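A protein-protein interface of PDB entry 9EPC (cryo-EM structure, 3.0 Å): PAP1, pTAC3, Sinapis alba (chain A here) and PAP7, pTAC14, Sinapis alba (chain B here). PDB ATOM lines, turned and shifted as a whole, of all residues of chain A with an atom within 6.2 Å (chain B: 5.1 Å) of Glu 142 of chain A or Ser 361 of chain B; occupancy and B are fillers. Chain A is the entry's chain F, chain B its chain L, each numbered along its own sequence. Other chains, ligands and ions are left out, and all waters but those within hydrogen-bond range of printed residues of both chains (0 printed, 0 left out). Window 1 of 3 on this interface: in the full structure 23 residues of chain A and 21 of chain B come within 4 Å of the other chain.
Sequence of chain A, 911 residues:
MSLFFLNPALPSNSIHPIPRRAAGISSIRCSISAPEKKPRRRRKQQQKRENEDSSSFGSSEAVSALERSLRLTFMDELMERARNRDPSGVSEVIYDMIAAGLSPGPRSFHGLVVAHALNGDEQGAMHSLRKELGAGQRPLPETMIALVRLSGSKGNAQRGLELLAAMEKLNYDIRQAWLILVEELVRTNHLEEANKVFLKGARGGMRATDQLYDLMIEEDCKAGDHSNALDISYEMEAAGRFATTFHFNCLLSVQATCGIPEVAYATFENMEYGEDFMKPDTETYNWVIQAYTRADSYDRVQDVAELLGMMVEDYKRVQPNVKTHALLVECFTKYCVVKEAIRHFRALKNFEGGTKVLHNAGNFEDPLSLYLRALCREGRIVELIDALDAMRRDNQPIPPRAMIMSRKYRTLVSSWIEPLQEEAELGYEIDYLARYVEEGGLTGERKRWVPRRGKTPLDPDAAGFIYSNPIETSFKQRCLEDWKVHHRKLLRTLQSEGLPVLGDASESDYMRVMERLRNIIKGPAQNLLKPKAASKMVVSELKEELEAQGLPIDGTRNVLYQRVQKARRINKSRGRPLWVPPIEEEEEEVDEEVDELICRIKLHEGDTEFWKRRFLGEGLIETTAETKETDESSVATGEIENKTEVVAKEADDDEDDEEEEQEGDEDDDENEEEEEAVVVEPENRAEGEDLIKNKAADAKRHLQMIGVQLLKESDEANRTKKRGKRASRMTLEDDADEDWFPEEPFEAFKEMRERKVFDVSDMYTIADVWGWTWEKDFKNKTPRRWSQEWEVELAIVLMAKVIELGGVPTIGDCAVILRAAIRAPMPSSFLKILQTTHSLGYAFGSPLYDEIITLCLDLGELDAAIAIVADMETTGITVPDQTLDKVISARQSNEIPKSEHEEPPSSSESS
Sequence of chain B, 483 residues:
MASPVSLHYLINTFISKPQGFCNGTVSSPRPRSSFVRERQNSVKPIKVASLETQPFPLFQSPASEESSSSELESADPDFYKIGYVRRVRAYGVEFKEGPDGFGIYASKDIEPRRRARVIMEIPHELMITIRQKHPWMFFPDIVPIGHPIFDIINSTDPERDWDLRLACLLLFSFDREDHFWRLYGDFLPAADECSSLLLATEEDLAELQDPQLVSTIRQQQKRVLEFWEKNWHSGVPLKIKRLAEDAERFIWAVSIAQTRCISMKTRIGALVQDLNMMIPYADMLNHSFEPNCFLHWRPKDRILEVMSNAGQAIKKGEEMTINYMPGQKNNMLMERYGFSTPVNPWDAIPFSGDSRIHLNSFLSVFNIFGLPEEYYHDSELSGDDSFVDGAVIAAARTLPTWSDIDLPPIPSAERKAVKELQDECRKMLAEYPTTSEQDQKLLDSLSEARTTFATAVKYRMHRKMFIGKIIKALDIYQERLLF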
ATOM      1  N   ARG A 107     -19.946   9.294  25.380  1.00  0.00           N
ATOM      2  CA  ARG A 107     -19.473   9.862  26.633  1.00  0.00           C
ATOM      3  C   ARG A 107     -20.006   9.112  27.845  1.00  0.00           C
ATOM      4  O   ARG A 107     -19.423   9.219  28.929  1.00  0.00           O
ATOM      5  CB  ARG A 107     -19.857  11.339  26.719  1.00  0.00           C
ATOM      6  CG  ARG A 107     -19.014  12.135  27.696  1.00  0.00           C
ATOM      7  CD  ARG A 107     -19.240  13.625  27.524  1.00  0.00           C
ATOM      8  NE  ARG A 107     -18.951  14.068  26.165  1.00  0.00           N
ATOM      9  CZ  ARG A 107     -17.759  14.464  25.744  1.00  0.00           C
ATOM     10  NH1 ARG A 107     -16.711  14.481  26.552  1.00  0.00           N
ATOM     11  NH2 ARG A 107     -17.612  14.847  24.479  1.00  0.00           N
ATOM     12  N   HIS A 110     -17.440   6.852  28.543  1.00  0.00           N
ATOM     13  CA  HIS A 110     -16.228   7.549  28.957  1.00  0.00           C
ATOM     14  C   HIS A 110     -16.036   7.464  30.465  1.00  0.00           C
ATOM     15  O   HIS A 110     -14.926   7.204  30.943  1.00  0.00           O
ATOM     16  CB  HIS A 110     -16.282   9.007  28.503  1.00  0.00           C
ATOM     17  CG  HIS A 110     -14.987   9.741  28.666  1.00  0.00           C
ATOM     18  ND1 HIS A 110     -13.814   9.112  29.022  1.00  0.00           N
ATOM     19  CD2 HIS A 110     -14.682  11.051  28.516  1.00  0.00           C
ATOM     20  CE1 HIS A 110     -12.841  10.003  29.085  1.00  0.00           C
ATOM     21  NE2 HIS A 110     -13.341  11.188  28.785  1.00  0.00           N
ATOM     22  N   VAL A 113     -15.120   3.885  31.235  1.00  0.00           N
ATOM     23  CA  VAL A 113     -13.750   3.555  30.855  1.00  0.00           C
ATOM     24  C   VAL A 113     -12.761   4.094  31.881  1.00  0.00           C
ATOM     25  O   VAL A 113     -11.860   3.378  32.331  1.00  0.00           O
ATOM     26  CB  VAL A 113     -13.447   4.084  29.441  1.00  0.00           C
ATOM     27  CG1 VAL A 113     -11.968   4.380  29.289  1.00  0.00           C
ATOM     28  CG2 VAL A 113     -13.895   3.077  28.397  1.00  0.00           C
ATOM     29  N   VAL A 114     -12.919   5.361  32.275  1.00  0.00           N
ATOM     30  CA  VAL A 114     -11.951   5.966  33.184  1.00  0.00           C
ATOM     31  C   VAL A 114     -12.000   5.302  34.552  1.00  0.00           C
ATOM     32  O   VAL A 114     -10.989   5.263  35.264  1.00  0.00           O
ATOM     33  CB  VAL A 114     -12.171   7.487  33.286  1.00  0.00           C
ATOM     34  CG1 VAL A 114     -11.980   8.142  31.929  1.00  0.00           C
ATOM     35  CG2 VAL A 114     -13.548   7.798  33.847  1.00  0.00           C
ATOM     36  N   LEU A 140     -15.064   8.226  22.083  1.00  0.00           N
ATOM     37  CA  LEU A 140     -14.475   9.551  22.169  1.00  0.00           C
ATOM     38  C   LEU A 140     -12.950   9.459  22.191  1.00  0.00           C
ATOM     39  O   LEU A 140     -12.384   8.496  22.716  1.00  0.00           O
ATOM     40  CB  LEU A 140     -14.965  10.275  23.417  1.00  0.00           C
ATOM     41  CG  LEU A 140     -16.442  10.664  23.443  1.00  0.00           C
ATOM     42  CD1 LEU A 140     -16.763  11.375  24.741  1.00  0.00           C
ATOM     43  CD2 LEU A 140     -16.782  11.539  22.251  1.00  0.00           C
ATOM     44  N   PRO A 141     -12.262  10.450  21.619  1.00  0.00           N
ATOM     45  CA  PRO A 141     -10.791  10.439  21.665  1.00  0.00           C
ATOM     46  C   PRO A 141     -10.228  10.433  23.073  1.00  0.00           C
ATOM     47  O   PRO A 141      -9.180   9.820  23.305  1.00  0.00           O
ATOM     48  CB  PRO A 141     -10.410  11.720  20.909  1.00  0.00           C
ATOM     49  CG  PRO A 141     -11.576  11.989  20.019  1.00  0.00           C
ATOM     50  CD  PRO A 141     -12.782  11.555  20.797  1.00  0.00           C
ATOM     51  N   GLU A 142     -10.890  11.099  24.023  1.00  0.00           N
ATOM     52  CA  GLU A 142     -10.416  11.075  25.403  1.00  0.00           C
ATOM     53  C   GLU A 142     -10.425   9.656  25.954  1.00  0.00           C
ATOM     54  O   GLU A 142      -9.505   9.255  26.676  1.00  0.00           O
ATOM     55  CB  GLU A 142     -11.271  11.989  26.279  1.00  0.00           C
ATOM     56  CG  GLU A 142     -11.489  13.384  25.726  1.00  0.00           C
ATOM     57  CD  GLU A 142     -12.714  13.474  24.840  1.00  0.00           C
ATOM     58  OE1 GLU A 142     -12.832  12.664  23.897  1.00  0.00           O
ATOM     59  OE2 GLU A 142     -13.565  14.352  25.093  1.00  0.00           O
ATOM     60  N   THR A 143     -11.464   8.884  25.626  1.00  0.00           N
ATOM     61  CA  THR A 143     -11.488   7.477  26.007  1.00  0.00           C
ATOM     62  C   THR A 143     -10.347   6.716  25.347  1.00  0.00           C
ATOM     63  O   THR A 143      -9.697   5.878  25.982  1.00  0.00           O
ATOM     64  CB  THR A 143     -12.828   6.854  25.621  1.00  0.00           C
ATOM     65  OG1 THR A 143     -12.874   6.660  24.203  1.00  0.00           O
ATOM     66  CG2 THR A 143     -13.967   7.767  26.021  1.00  0.00           C
ATOM     67  N   MET A 144     -10.090   6.996  24.069  1.00  0.00           N
ATOM     68  CA  MET A 144      -9.002   6.329  23.367  1.00  0.00           C
ATOM     69  C   MET A 144      -7.650   6.704  23.958  1.00  0.00           C
ATOM     70  O   MET A 144      -6.776   5.845  24.120  1.00  0.00           O
ATOM     71  CB  MET A 144      -9.060   6.678  21.882  1.00  0.00           C
ATOM     72  CG  MET A 144     -10.403   6.392  21.246  1.00  0.00           C
ATOM     73  SD  MET A 144     -10.817   4.644  21.321  1.00  0.00           S
ATOM     74  CE  MET A 144      -9.483   3.954  20.352  1.00  0.00           C
ATOM     75  N   ILE A 145      -7.462   7.983  24.291  1.00  0.00           N
ATOM     76  CA  ILE A 145      -6.202   8.425  24.880  1.00  0.00           C
ATOM     77  C   ILE A 145      -5.991   7.771  26.239  1.00  0.00           C
ATOM     78  O   ILE A 145      -4.877   7.355  26.580  1.00  0.00           O
ATOM     79  CB  ILE A 145      -6.171   9.961  24.973  1.00  0.00           C
ATOM     80  CG1 ILE A 145      -6.062  10.573  23.575  1.00  0.00           C
ATOM     81  CG2 ILE A 145      -5.026  10.427  25.855  1.00  0.00           C
ATOM     82  CD1 ILE A 145      -6.002  12.081  23.568  1.00  0.00           C
ATOM     83  N   ALA A 146      -7.056   7.665  27.037  1.00  0.00           N
ATOM     84  CA  ALA A 146      -6.936   7.017  28.337  1.00  0.00           C
ATOM     85  C   ALA A 146      -6.585   5.543  28.198  1.00  0.00           C
ATOM     86  O   ALA A 146      -5.882   4.990  29.051  1.00  0.00           O
ATOM     87  CB  ALA A 146      -8.231   7.182  29.129  1.00  0.00           C
ATOM     88  N   LEU A 147      -7.065   4.891  27.138  1.00  0.00           N
ATOM     89  CA  LEU A 147      -6.778   3.474  26.946  1.00  0.00           C
ATOM     90  C   LEU A 147      -5.288   3.235  26.733  1.00  0.00           C
ATOM     91  O   LEU A 147      -4.680   2.392  27.403  1.00  0.00           O
ATOM     92  CB  LEU A 147      -7.585   2.936  25.765  1.00  0.00           C
ATOM     93  CG  LEU A 147      -8.785   2.045  26.093  1.00  0.00           C
ATOM     94  CD1 LEU A 147      -8.333   0.794  26.823  1.00  0.00           C
ATOM     95  CD2 LEU A 147      -9.805   2.798  26.917  1.00  0.00           C
ATOM     96  N   ARG A 149      -2.784   5.224  27.402  1.00  0.00           N
ATOM     97  CA  ARG A 149      -2.030   5.622  28.584  1.00  0.00           C
ATOM     98  C   ARG A 149      -2.053   4.527  29.642  1.00  0.00           C
ATOM     99  O   ARG A 149      -1.035   4.253  30.288  1.00  0.00           O
ATOM    100  CB  ARG A 149      -2.583   6.926  29.155  1.00  0.00           C
ATOM    101  CG  ARG A 149      -1.959   7.311  30.482  1.00  0.00           C
ATOM    102  CD  ARG A 149      -2.583   8.561  31.062  1.00  0.00           C
ATOM    103  NE  ARG A 149      -2.186   9.768  30.349  1.00  0.00           N
ATOM    104  CZ  ARG A 149      -2.937  10.390  29.451  1.00  0.00           C
ATOM    105  NH1 ARG A 149      -4.137   9.940  29.123  1.00  0.00           N
ATOM    106  NH2 ARG A 149      -2.474  11.493  28.870  1.00  0.00           N
ATOM    107  N   HIS B 358     -13.132  21.547  31.541  1.00  0.00           N
ATOM    108  CA  HIS B 358     -12.249  20.494  31.046  1.00  0.00           C
ATOM    109  C   HIS B 358     -12.077  20.698  29.546  1.00  0.00           C
ATOM    110  O   HIS B 358     -12.968  20.376  28.757  1.00  0.00           O
ATOM    111  CB  HIS B 358     -12.819  19.118  31.365  1.00  0.00           C
ATOM    112  CG  HIS B 358     -11.850  18.000  31.149  1.00  0.00           C
ATOM    113  ND1 HIS B 358     -10.692  17.869  31.885  1.00  0.00           N
ATOM    114  CD2 HIS B 358     -11.863  16.963  30.280  1.00  0.00           C
ATOM    115  CE1 HIS B 358     -10.034  16.798  31.480  1.00  0.00           C
ATOM    116  NE2 HIS B 358     -10.724  16.230  30.507  1.00  0.00           N
ATOM    117  N   LEU B 359     -10.921  21.237  29.149  1.00  0.00           N
ATOM    118  CA  LEU B 359     -10.713  21.576  27.746  1.00  0.00           C
ATOM    119  C   LEU B 359     -10.662  20.337  26.864  1.00  0.00           C
ATOM    120  O   LEU B 359     -10.998  20.411  25.677  1.00  0.00           O
ATOM    121  CB  LEU B 359      -9.434  22.397  27.575  1.00  0.00           C
ATOM    122  CG  LEU B 359      -8.091  21.716  27.834  1.00  0.00           C
ATOM    123  CD1 LEU B 359      -7.020  22.331  26.951  1.00  0.00           C
ATOM    124  CD2 LEU B 359      -7.697  21.834  29.293  1.00  0.00           C
ATOM    125  N   ASN B 360     -10.249  19.193  27.417  1.00  0.00           N
ATOM    126  CA  ASN B 360     -10.195  17.972  26.620  1.00  0.00           C
ATOM    127  C   ASN B 360     -11.573  17.608  26.088  1.00  0.00           C
ATOM    128  O   ASN B 360     -11.716  17.230  24.920  1.00  0.00           O
ATOM    129  CB  ASN B 360      -9.621  16.826  27.451  1.00  0.00           C
ATOM    130  CG  ASN B 360      -8.224  17.116  27.952  1.00  0.00           C
ATOM    131  OD1 ASN B 360      -8.043  17.648  29.046  1.00  0.00           O
ATOM    132  ND2 ASN B 360      -7.224  16.769  27.150  1.00  0.00           N
ATOM    133  N   SER B 361     -12.599  17.718  26.932  1.00  0.00           N
ATOM    134  CA  SER B 361     -13.966  17.576  26.448  1.00  0.00           C
ATOM    135  C   SER B 361     -14.301  18.673  25.448  1.00  0.00           C
ATOM    136  O   SER B 361     -14.948  18.419  24.425  1.00  0.00           O
ATOM    137  CB  SER B 361     -14.940  17.604  27.623  1.00  0.00           C
ATOM    138  OG  SER B 361     -14.787  18.797  28.374  1.00  0.00           O
ATOM    139  N   PHE B 362     -13.866  19.902  25.729  1.00  0.00           N
ATOM    140  CA  PHE B 362     -14.113  21.009  24.811  1.00  0.00           C
ATOM    141  C   PHE B 362     -13.395  20.802  23.483  1.00  0.00           C
ATOM    142  O   PHE B 362     -13.942  21.117  22.420  1.00  0.00           O
ATOM    143  CB  PHE B 362     -13.682  22.323  25.458  1.00  0.00           C
ATOM    144  CG  PHE B 362     -13.783  23.507  24.547  1.00  0.00           C
ATOM    145  CD1 PHE B 362     -14.996  24.141  24.349  1.00  0.00           C
ATOM    146  CD2 PHE B 362     -12.664  23.991  23.891  1.00  0.00           C
ATOM    147  CE1 PHE B 362     -15.091  25.233  23.512  1.00  0.00           C
ATOM    148  CE2 PHE B 362     -12.754  25.081  23.052  1.00  0.00           C
ATOM    149  CZ  PHE B 362     -13.970  25.703  22.862  1.00  0.00           C
ATOM    150  N   LEU B 363     -12.163  20.291  23.523  1.00  0.00           N
ATOM    151  CA  LEU B 363     -11.418  20.061  22.289  1.00  0.00           C
ATOM    152  C   LEU B 363     -12.083  18.992  21.431  1.00  0.00           C
ATOM    153  O   LEU B 363     -12.212  19.151  20.212  1.00  0.00           O
ATOM    154  CB  LEU B 363      -9.977  19.667  22.612  1.00  0.00           C
ATOM    155  CG  LEU B 363      -9.070  20.749  23.199  1.00  0.00           C
ATOM    156  CD1 LEU B 363      -7.714  20.169  23.568  1.00  0.00           C
ATOM    157  CD2 LEU B 363      -8.914  21.896  22.220  1.00  0.00           C
ATOM    158  N   SER B 364     -12.518  17.896  22.054  1.00  0.00           N
ATOM    159  CA  SER B 364     -13.040  16.771  21.287  1.00  0.00           C
ATOM    160  C   SER B 364     -14.413  17.062  20.703  1.00  0.00           C
ATOM    161  O   SER B 364     -14.720  16.606  19.595  1.00  0.00           O
ATOM    162  CB  SER B 364     -13.101  15.524  22.165  1.00  0.00           C
ATOM    163  OG  SER B 364     -13.991  15.721  23.249  1.00  0.00           O
ATOM    164  N   VAL B 365     -15.254  17.807  21.424  1.00  0.00           N
ATOM    165  CA  VAL B 365     -16.615  18.048  20.964  1.00  0.00           C
ATOM    166  C   VAL B 365     -16.632  18.848  19.669  1.00  0.00           C
ATOM    167  O   VAL B 365     -17.603  18.775  18.908  1.00  0.00           O
ATOM    168  CB  VAL B 365     -17.437  18.743  22.073  1.00  0.00           C
ATOM    169  CG1 VAL B 365     -16.961  20.166  22.287  1.00  0.00           C
ATOM    170  CG2 VAL B 365     -18.919  18.711  21.743  1.00  0.00           C
ATOM    171  N   ASP B 406      -6.520  11.893  33.540  1.00  0.00           N
ATOM    172  CA  ASP B 406      -7.708  11.453  32.819  1.00  0.00           C
ATOM    173  C   ASP B 406      -9.006  11.803  33.536  1.00  0.00           C
ATOM    174  O   ASP B 406     -10.052  11.252  33.170  1.00  0.00           O
ATOM    175  CB  ASP B 406      -7.647   9.941  32.564  1.00  0.00           C
ATOM    176  CG  ASP B 406      -6.755   9.582  31.393  1.00  0.00           C
ATOM    177  OD1 ASP B 406      -6.796  10.301  30.372  1.00  0.00           O
ATOM    178  OD2 ASP B 406      -6.011   8.585  31.491  1.00  0.00           O
ATOM    179  N   PRO B 409     -14.834  15.313  33.743  1.00  0.00           N
ATOM    180  CA  PRO B 409     -15.447  16.493  34.355  1.00  0.00           C
ATOM    181  C   PRO B 409     -16.833  16.183  34.907  1.00  0.00           C
ATOM    182  O   PRO B 409     -17.434  15.147  34.625  1.00  0.00           O
ATOM    183  CB  PRO B 409     -15.525  17.483  33.193  1.00  0.00           C
ATOM    184  CG  PRO B 409     -15.705  16.607  31.998  1.00  0.00           C
ATOM    185  CD  PRO B 409     -14.920  15.346  32.272  1.00  0.00           C
ATOM    186  N   GLU B 414     -19.824  21.983  35.451  1.00  0.00           N
ATOM    187  CA  GLU B 414     -19.575  22.765  34.247  1.00  0.00           C
ATOM    188  C   GLU B 414     -20.833  23.503  33.805  1.00  0.00           C
ATOM    189  O   GLU B 414     -20.766  24.676  33.426  1.00  0.00           O
ATOM    190  CB  GLU B 414     -19.042  21.866  33.133  1.00  0.00           C
ATOM    191  CG  GLU B 414     -17.667  21.284  33.430  1.00  0.00           C
ATOM    192  CD  GLU B 414     -16.942  20.816  32.184  1.00  0.00           C
ATOM    193  OE1 GLU B 414     -17.596  20.679  31.130  1.00  0.00           O
ATOM    194  OE2 GLU B 414     -15.714  20.594  32.256  1.00  0.00           O
ATOM    195  N   TYR B 477     -21.416  23.515  23.392  1.00  0.00           N
ATOM    196  CA  TYR B 477     -20.579  22.630  24.196  1.00  0.00           C
ATOM    197  C   TYR B 477     -21.322  22.131  25.428  1.00  0.00           C
ATOM    198  O   TYR B 477     -21.203  20.958  25.801  1.00  0.00           O
ATOM    199  CB  TYR B 477     -19.295  23.352  24.601  1.00  0.00           C
ATOM    200  CG  TYR B 477     -18.590  22.743  25.791  1.00  0.00           C
ATOM    201  CD1 TYR B 477     -17.796  21.613  25.649  1.00  0.00           C
ATOM    202  CD2 TYR B 477     -18.706  23.307  27.055  1.00  0.00           C
ATOM    203  CE1 TYR B 477     -17.146  21.057  26.734  1.00  0.00           C
ATOM    204  CE2 TYR B 477     -18.061  22.758  28.143  1.00  0.00           C
ATOM    205  CZ  TYR B 477     -17.282  21.634  27.978  1.00  0.00           C
ATOM    206  OH  TYR B 477     -16.638  21.084  29.061  1.00  0.00           O
ATOM    207  N   LEU B 481     -22.307  18.128  25.929  1.00  0.00           N
ATOM    208  CA  LEU B 481     -21.617  17.381  26.973  1.00  0.00           C
ATOM    209  C   LEU B 481     -22.477  16.249  27.518  1.00  0.00           C
ATOM    210  O   LEU B 481     -21.944  15.238  27.989  1.00  0.00           O
ATOM    211  CB  LEU B 481     -21.204  18.327  28.101  1.00  0.00           C
ATOM    212  CG  LEU B 481     -20.353  17.731  29.221  1.00  0.00           C
ATOM    213  CD1 LEU B 481     -19.039  17.205  28.669  1.00  0.00           C
ATOM    214  CD2 LEU B 481     -20.109  18.760  30.310  1.00  0.00           C
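Of chain B, only Asn 360 (3.4 Å), Ser 361 (3.5 Å) and Ser 364 (2.3 Å) come within 4 Å of Glu 142 of chain A.
Ser 361 of chain B touches two residues of chain A.
Printed residues of chain A within 4 Å of Asn 360 of chain B: Glu 142.
Printed residues of chain B within 4 Å of Arg 107 of chain A: Ser 361 (3.7 Å), Ser 364 (3.9 Å) and Leu 481 (3.2 Å).
Of the printed residues of chain A, Leu 481 of chain B touches Arg 107.
Printed residues of chain B within 4 Å of Ala 146 of chain A: Asp 406.
Val 113 of chain A touches none of the printed residues of chain B.
Leu 140 of chain A touches none of the printed residues of chain B.
The side-chain carboxylate (OD1) of Asp 406 of chain B lies within salt-bridge range of the guanidinium group (NH1) of Arg 149 of chain A.
The side-chain carboxylate (OE1) of Glu 142 of chain A sits close to the side-chain hydroxyl (OG) of Ser 364 of chain B (3.3 Å).
The side-chain carboxylate (OE2) of Glu 142 of chain A sits close to the backbone carbonyl oxygen (O) of Asn 360 of chain B, at 3.4 Å.
Among the printed residues, merely in contact across the chains: Arg 107 of chain A with Leu 481 of chain B, Glu 142 of chain A with Ser 361 of chain B, Ala 146 of chain A with Asp 406 of chain B, Arg 107 of chain A with Ser 361 of chain B, Val 114 of chain A with Asp 406 of chain B and Arg 107 of chain A with Ser 364 of chain B.
The side-chain hydroxyl (OG) of Ser 361 of chain B lies within hydrogen-bond range of the side-chain hydroxyl (OH) of Tyr 477 of chain B (3.0 Å).
O of Asn 360 of chain B lies within hydrogen-bond range of OG of Ser 364 of chain B, 3.2 Å away.
The backbone carbonyl oxygen of Ser 361 of chain B lies within hydrogen-bond range of the side-chain hydroxyl of Ser 364 of chain B (3.1 Å).
A ring nitrogen (NE2) of His 358 of chain B lies close to the side-chain amide oxygen (OD1) of Asn 360 of chain B, 3.4 Å away.
OG of Ser 361 of chain B lies within hydrogen-bond range of O of His 358 of chain B (2.4 Å).
OE2 of Glu 142 of chain A lies within salt-bridge range of NH1 of Arg 107 of chain A, 3.5 Å away.
Of the 13 printed residues of chain A, 5 touch a printed residue of chain B.
Printed residues of chain A that touch a printed residue of chain B: Arg 107, Val 114, Glu 142, Ala 146 and Arg 149.
Along chain A the printed residues that touch a printed residue of chain B span positions 107 to 149.
Of the 13 printed residues of chain B, 5 touch a printed residue of chain A.
Among the printed residues, Asp or Glu carboxylates within 4 Å of a Lys or Arg side-chain nitrogen of the other chain: Arg 149 of chain A with Asp 406 of chain B.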
